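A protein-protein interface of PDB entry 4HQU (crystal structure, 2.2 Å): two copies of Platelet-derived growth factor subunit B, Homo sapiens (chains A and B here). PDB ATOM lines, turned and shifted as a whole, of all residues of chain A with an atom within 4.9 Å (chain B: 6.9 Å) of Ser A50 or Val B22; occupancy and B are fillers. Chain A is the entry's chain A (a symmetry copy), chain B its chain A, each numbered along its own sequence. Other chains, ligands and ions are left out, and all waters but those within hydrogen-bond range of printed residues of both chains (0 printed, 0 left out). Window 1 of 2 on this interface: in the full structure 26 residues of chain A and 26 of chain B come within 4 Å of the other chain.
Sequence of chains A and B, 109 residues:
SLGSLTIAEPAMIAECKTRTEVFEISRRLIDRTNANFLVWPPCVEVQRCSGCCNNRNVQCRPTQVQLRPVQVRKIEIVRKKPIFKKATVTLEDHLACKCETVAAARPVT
Positions printed for both chains: 21 and 48.
Among the printed residues, pairs that only touch across the chains: Arg A19 with Val B22, Ala A14 with Val B44, Ser A50 with Val B22, Gly A51 with Val B22 and Ala A14 with Glu B45.
NH1 of Arg A19 sits at hydrogen-bond distance from O of Ser A50, 2.6 Å away. The backbone carbonyl oxygen of Val B44 lies within hydrogen-bond range of the backbone NH of Phe B23, 2.7 Å away. SG of Cys A60 forms a disulfide with SG of Cys A16, 2.1 Å away. The backbone carbonyl oxygen (O) of Glu A15 sits at hydrogen-bond distance from the guanidinium group (NH2) of Arg A19. The backbone NH (N) of Arg A19 sits at hydrogen-bond distance from the backbone carbonyl oxygen (O) of Arg A48 (2.8 Å). The backbone carbonyl oxygen of Lys A17 sits at hydrogen-bond distance from the backbone NH of Ser A50.
Printed residues of chain B within 4 Å of Lys A17: Glu B45. Printed residues of chain B within 4 Å of Arg A19: Val B22 (3.7 Å) and Glu B45 (2.9 Å). Of chain B, only Val B22 (3.8 Å) comes within 4 Å of Ser A50. Printed residues of chain B within 4 Å of Gly A51: Val B22. Of the printed residues of chain B, Cys A52 touches Cys B43 (2.2 Å). Printed residues of chain A within 4 Å of Val B22: Arg A19 (3.7 Å), Ser A50 (3.8 Å) and Gly A51 (3.8 Å). Of the printed residues of chain A, Glu B45 touches Ala A14 (3.99 Å), Lys A17 (3.5 Å) and Arg A19 (2.9 Å). The nearest residue of chain A that does not touch Val B22 is Ala A14 (4.1 Å).
NE of Arg A19 lies within salt-bridge range of OE2 of Glu B45 (2.9 Å). SG of Cys B43 is disulfide-bonded to SG of Cys A52 (2.2 Å). O of Cys B43 is in hydrogen-bond range of N of Ala A14 (2.9 Å). OE2 of Glu B45 is in salt-bridge range of NZ of Lys A17 (3.6 Å).
Of the 10 printed residues of chain B, 4 touch a printed residue of chain A. Hydrophobic or aromatic side chains of chain B within 4 Å of the printed part of chain A: Val B22. Of the 12 printed residues of chain A, 6 touch a printed residue of chain B. Hydrophobic or aromatic side chains of chain A that line the printed part of chain B: Ala A14.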
ATOM      1  N   ALA A  14       6.657 -23.874  19.974  1.00  0.00           N
ATOM      2  CA  ALA A  14       5.529 -23.977  19.058  1.00  0.00           C
ATOM      3  C   ALA A  14       4.508 -24.840  19.771  1.00  0.00           C
ATOM      4  O   ALA A  14       4.647 -26.076  19.834  1.00  0.00           O
ATOM      5  CB  ALA A  14       5.963 -24.604  17.744  1.00  0.00           C
ATOM      6  N   GLU A  15       3.503 -24.172  20.337  1.00  0.00           N
ATOM      7  CA  GLU A  15       2.447 -24.809  21.120  1.00  0.00           C
ATOM      8  C   GLU A  15       1.626 -25.749  20.246  1.00  0.00           C
ATOM      9  O   GLU A  15       1.572 -25.586  19.010  1.00  0.00           O
ATOM     10  CB  GLU A  15       1.536 -23.746  21.769  1.00  0.00           C
ATOM     11  N   CYS A  16       1.035 -26.751  20.892  1.00  0.00           N
ATOM     12  CA  CYS A  16       0.096 -27.646  20.254  1.00  0.00           C
ATOM     13  C   CYS A  16      -1.165 -26.846  20.016  1.00  0.00           C
ATOM     14  O   CYS A  16      -1.860 -26.501  20.970  1.00  0.00           O
ATOM     15  CB  CYS A  16      -0.199 -28.847  21.148  1.00  0.00           C
ATOM     16  SG  CYS A  16      -1.581 -29.874  20.589  1.00  0.00           S
ATOM     17  N   LYS A  17      -1.420 -26.510  18.752  1.00  0.00           N
ATOM     18  CA  LYS A  17      -2.625 -25.779  18.355  1.00  0.00           C
ATOM     19  C   LYS A  17      -2.898 -25.989  16.867  1.00  0.00           C
ATOM     20  O   LYS A  17      -2.086 -26.592  16.153  1.00  0.00           O
ATOM     21  CB  LYS A  17      -2.473 -24.279  18.631  1.00  0.00           C
ATOM     22  CG  LYS A  17      -1.369 -23.603  17.834  1.00  0.00           C
ATOM     23  CD  LYS A  17      -1.416 -22.098  18.003  1.00  0.00           C
ATOM     24  CE  LYS A  17      -0.316 -21.459  17.187  1.00  0.00           C
ATOM     25  NZ  LYS A  17      -0.215 -19.996  17.433  1.00  0.00           N
ATOM     26  N   ARG A  19      -2.998 -24.941  13.058  1.00  0.00           N
ATOM     27  CA  ARG A  19      -2.330 -24.075  12.093  1.00  0.00           C
ATOM     28  C   ARG A  19      -2.830 -24.425  10.688  1.00  0.00           C
ATOM     29  O   ARG A  19      -3.367 -25.509  10.456  1.00  0.00           O
ATOM     30  CB  ARG A  19      -0.811 -24.260  12.157  1.00  0.00           C
ATOM     31  CG  ARG A  19      -0.164 -23.737  13.436  1.00  0.00           C
ATOM     32  CD  ARG A  19       1.331 -24.052  13.523  1.00  0.00           C
ATOM     33  NE  ARG A  19       1.869 -23.595  14.801  1.00  0.00           N
ATOM     34  CZ  ARG A  19       1.836 -24.295  15.937  1.00  0.00           C
ATOM     35  NH1 ARG A  19       1.318 -25.530  15.977  1.00  0.00           N
ATOM     36  NH2 ARG A  19       2.339 -23.761  17.051  1.00  0.00           N
ATOM     37  N   GLU A  21      -2.526 -25.744   7.116  1.00  0.00           N
ATOM     38  CA  GLU A  21      -1.686 -26.612   6.295  1.00  0.00           C
ATOM     39  C   GLU A  21      -2.238 -26.744   4.868  1.00  0.00           C
ATOM     40  O   GLU A  21      -3.368 -26.307   4.580  1.00  0.00           O
ATOM     41  CB  GLU A  21      -1.545 -27.983   6.952  1.00  0.00           C
ATOM     42  CG  GLU A  21      -0.670 -27.939   8.201  1.00  0.00           C
ATOM     43  CD  GLU A  21      -0.415 -29.304   8.797  1.00  0.00           C
ATOM     44  OE1 GLU A  21      -0.810 -30.314   8.186  1.00  0.00           O
ATOM     45  OE2 GLU A  21       0.190 -29.370   9.881  1.00  0.00           O
ATOM     46  N   ARG A  48      -5.054 -27.729  10.868  1.00  0.00           N
ATOM     47  CA  ARG A  48      -4.558 -28.977  11.452  1.00  0.00           C
ATOM     48  C   ARG A  48      -3.808 -28.753  12.775  1.00  0.00           C
ATOM     49  O   ARG A  48      -3.176 -27.703  12.989  1.00  0.00           O
ATOM     50  CB  ARG A  48      -3.661 -29.732  10.449  1.00  0.00           C
ATOM     51  CG  ARG A  48      -4.378 -30.302   9.218  1.00  0.00           C
ATOM     52  CD  ARG A  48      -5.351 -31.431   9.572  1.00  0.00           C
ATOM     53  NE  ARG A  48      -6.337 -31.721   8.514  1.00  0.00           N
ATOM     54  CZ  ARG A  48      -6.187 -32.682   7.609  1.00  0.00           C
ATOM     55  NH1 ARG A  48      -5.096 -33.442   7.626  1.00  0.00           N
ATOM     56  NH2 ARG A  48      -7.113 -32.893   6.684  1.00  0.00           N
ATOM     57  N   CYS A  49      -3.897 -29.747  13.656  1.00  0.00           N
ATOM     58  CA  CYS A  49      -3.210 -29.724  14.932  1.00  0.00           C
ATOM     59  C   CYS A  49      -1.752 -29.996  14.660  1.00  0.00           C
ATOM     60  O   CYS A  49      -1.423 -30.981  14.022  1.00  0.00           O
ATOM     61  CB  CYS A  49      -3.784 -30.789  15.873  1.00  0.00           C
ATOM     62  SG  CYS A  49      -5.426 -30.342  16.508  1.00  0.00           S
ATOM     63  N   SER A  50      -0.889 -29.088  15.101  1.00  0.00           N
ATOM     64  CA  SER A  50       0.539 -29.299  15.024  1.00  0.00           C
ATOM     65  C   SER A  50       1.196 -28.620  16.227  1.00  0.00           C
ATOM     66  O   SER A  50       0.565 -27.827  16.935  1.00  0.00           O
ATOM     67  CB  SER A  50       1.088 -28.714  13.728  1.00  0.00           C
ATOM     68  OG  SER A  50       0.905 -27.308  13.745  1.00  0.00           O
ATOM     69  N   GLY A  51       2.471 -28.901  16.432  1.00  0.00           N
ATOM     70  CA  GLY A  51       3.212 -28.306  17.531  1.00  0.00           C
ATOM     71  C   GLY A  51       3.711 -29.398  18.445  1.00  0.00           C
ATOM     72  O   GLY A  51       3.454 -30.586  18.216  1.00  0.00           O
ATOM     73  N   CYS A  52       4.419 -29.005  19.494  1.00  0.00           N
ATOM     74  CA  CYS A  52       5.066 -29.983  20.360  1.00  0.00           C
ATOM     75  C   CYS A  52       4.596 -29.913  21.792  1.00  0.00           C
ATOM     76  O   CYS A  52       4.461 -28.834  22.356  1.00  0.00           O
ATOM     77  CB  CYS A  52       6.574 -29.813  20.290  1.00  0.00           C
ATOM     78  SG  CYS A  52       7.103 -30.000  18.581  1.00  0.00           S
ATOM     79  N   CYS A  60       0.363 -34.197  20.040  1.00  0.00           N
ATOM     80  CA  CYS A  60      -0.634 -33.195  19.701  1.00  0.00           C
ATOM     81  C   CYS A  60      -1.698 -33.790  18.764  1.00  0.00           C
ATOM     82  O   CYS A  60      -1.384 -34.201  17.649  1.00  0.00           O
ATOM     83  CB  CYS A  60       0.064 -32.012  19.041  1.00  0.00           C
ATOM     84  SG  CYS A  60      -0.987 -30.595  18.755  1.00  0.00           S
ATOM     85  N   THR B  20       3.104 -20.538   8.262  1.00  0.00           N
ATOM     86  CA  THR B  20       3.778 -20.876   9.512  1.00  0.00           C
ATOM     87  C   THR B  20       3.872 -22.386   9.689  1.00  0.00           C
ATOM     88  O   THR B  20       2.863 -23.070   9.694  1.00  0.00           O
ATOM     89  CB  THR B  20       3.032 -20.242  10.687  1.00  0.00           C
ATOM     90  OG1 THR B  20       3.043 -18.823  10.507  1.00  0.00           O
ATOM     91  CG2 THR B  20       3.697 -20.600  12.025  1.00  0.00           C
ATOM     92  N   GLU B  21       5.090 -22.899   9.817  1.00  0.00           N
ATOM     93  CA  GLU B  21       5.295 -24.318  10.100  1.00  0.00           C
ATOM     94  C   GLU B  21       6.002 -24.527  11.447  1.00  0.00           C
ATOM     95  O   GLU B  21       6.492 -23.562  12.065  1.00  0.00           O
ATOM     96  CB  GLU B  21       6.080 -24.973   8.967  1.00  0.00           C
ATOM     97  CG  GLU B  21       5.249 -25.116   7.695  1.00  0.00           C
ATOM     98  CD  GLU B  21       5.964 -25.873   6.600  1.00  0.00           C
ATOM     99  OE1 GLU B  21       7.062 -26.403   6.848  1.00  0.00           O
ATOM    100  OE2 GLU B  21       5.422 -25.945   5.483  1.00  0.00           O
ATOM    101  N   VAL B  22       6.049 -25.781  11.889  1.00  0.00           N
ATOM    102  CA  VAL B  22       6.695 -26.137  13.146  1.00  0.00           C
ATOM    103  C   VAL B  22       8.080 -26.708  12.844  1.00  0.00           C
ATOM    104  O   VAL B  22       8.196 -27.674  12.100  1.00  0.00           O
ATOM    105  CB  VAL B  22       5.827 -27.141  13.943  1.00  0.00           C
ATOM    106  CG1 VAL B  22       6.575 -27.702  15.152  1.00  0.00           C
ATOM    107  CG2 VAL B  22       4.539 -26.459  14.386  1.00  0.00           C
ATOM    108  N   PHE B  23       9.122 -26.093  13.405  1.00  0.00           N
ATOM    109  CA  PHE B  23      10.503 -26.554  13.233  1.00  0.00           C
ATOM    110  C   PHE B  23      11.030 -27.208  14.513  1.00  0.00           C
ATOM    111  O   PHE B  23      11.067 -26.589  15.565  1.00  0.00           O
ATOM    112  CB  PHE B  23      11.403 -25.378  12.833  1.00  0.00           C
ATOM    113  CG  PHE B  23      12.867 -25.738  12.668  1.00  0.00           C
ATOM    114  CD1 PHE B  23      13.795 -25.401  13.652  1.00  0.00           C
ATOM    115  CD2 PHE B  23      13.321 -26.396  11.522  1.00  0.00           C
ATOM    116  CE1 PHE B  23      15.143 -25.727  13.509  1.00  0.00           C
ATOM    117  CE2 PHE B  23      14.669 -26.719  11.366  1.00  0.00           C
ATOM    118  CZ  PHE B  23      15.582 -26.387  12.368  1.00  0.00           C
ATOM    119  N   GLU B  24      11.450 -28.458  14.420  1.00  0.00           N
ATOM    120  CA  GLU B  24      11.967 -29.147  15.573  1.00  0.00           C
ATOM    121  C   GLU B  24      13.448 -28.802  15.740  1.00  0.00           C
ATOM    122  O   GLU B  24      14.234 -28.880  14.779  1.00  0.00           O
ATOM    123  CB  GLU B  24      11.755 -30.644  15.418  1.00  0.00           C
ATOM    124  CG  GLU B  24      11.981 -31.432  16.693  1.00  0.00           C
ATOM    125  CD  GLU B  24      11.705 -32.914  16.516  1.00  0.00           C
ATOM    126  OE1 GLU B  24      10.877 -33.272  15.643  1.00  0.00           O
ATOM    127  OE2 GLU B  24      12.308 -33.717  17.262  1.00  0.00           O
ATOM    128  N   CYS B  43      10.723 -27.205  19.949  1.00  0.00           N
ATOM    129  CA  CYS B  43      10.246 -26.746  18.629  1.00  0.00           C
ATOM    130  C   CYS B  43       9.824 -25.297  18.629  1.00  0.00           C
ATOM    131  O   CYS B  43       9.334 -24.800  19.639  1.00  0.00           O
ATOM    132  CB  CYS B  43       9.021 -27.540  18.191  1.00  0.00           C
ATOM    133  SG  CYS B  43       9.206 -29.320  18.398  1.00  0.00           S
ATOM    134  N   VAL B  44       9.966 -24.647  17.473  1.00  0.00           N
ATOM    135  CA  VAL B  44       9.624 -23.241  17.296  1.00  0.00           C
ATOM    136  C   VAL B  44       8.875 -23.061  15.964  1.00  0.00           C
ATOM    137  O   VAL B  44       8.901 -23.938  15.098  1.00  0.00           O
ATOM    138  CB  VAL B  44      10.883 -22.341  17.286  1.00  0.00           C
ATOM    139  CG1 VAL B  44      11.553 -22.324  18.658  1.00  0.00           C
ATOM    140  CG2 VAL B  44      11.868 -22.818  16.224  1.00  0.00           C
ATOM    141  N   GLU B  45       8.204 -21.930  15.817  1.00  0.00           N
ATOM    142  CA  GLU B  45       7.529 -21.624  14.572  1.00  0.00           C
ATOM    143  C   GLU B  45       8.539 -21.034  13.619  1.00  0.00           C
ATOM    144  O   GLU B  45       9.419 -20.276  14.027  1.00  0.00           O
ATOM    145  CB  GLU B  45       6.361 -20.662  14.796  1.00  0.00           C
ATOM    146  CG  GLU B  45       5.180 -21.319  15.489  1.00  0.00           C
ATOM    147  CD  GLU B  45       3.942 -20.440  15.583  1.00  0.00           C
ATOM    148  OE1 GLU B  45       4.053 -19.201  15.470  1.00  0.00           O
ATOM    149  OE2 GLU B  45       2.842 -21.003  15.772  1.00  0.00           O
ATOM    150  N   VAL B  46       8.443 -21.426  12.357  1.00  0.00           N
ATOM    151  CA  VAL B  46       9.181 -20.778  11.287  1.00  0.00           C
ATOM    152  C   VAL B  46       8.224 -20.524  10.122  1.00  0.00           C
ATOM    153  O   VAL B  46       7.148 -21.123  10.054  1.00  0.00           O
ATOM    154  CB  VAL B  46      10.398 -21.594  10.803  1.00  0.00           C
ATOM    155  CG1 VAL B  46      11.461 -21.688  11.894  1.00  0.00           C
ATOM    156  CG2 VAL B  46       9.986 -22.982  10.320  1.00  0.00           C
ATOM    157  N   ARG B  48       7.580 -20.831   6.085  1.00  0.00           N
ATOM    158  CA  ARG B  48       8.051 -21.700   5.003  1.00  0.00           C
ATOM    159  C   ARG B  48       7.161 -21.619   3.751  1.00  0.00           C
ATOM    160  O   ARG B  48       5.943 -21.385   3.839  1.00  0.00           O
ATOM    161  CB  ARG B  48       8.166 -23.160   5.485  1.00  0.00           C
ATOM    162  CG  ARG B  48       9.268 -23.433   6.517  1.00  0.00           C
ATOM    163  CD  ARG B  48      10.676 -23.255   5.941  1.00  0.00           C
ATOM    164  NE  ARG B  48      11.726 -23.104   6.965  1.00  0.00           N
ATOM    165  CZ  ARG B  48      12.473 -24.109   7.408  1.00  0.00           C
ATOM    166  NH1 ARG B  48      12.289 -25.334   6.924  1.00  0.00           N
ATOM    167  NH2 ARG B  48      13.403 -23.907   8.331  1.00  0.00           N
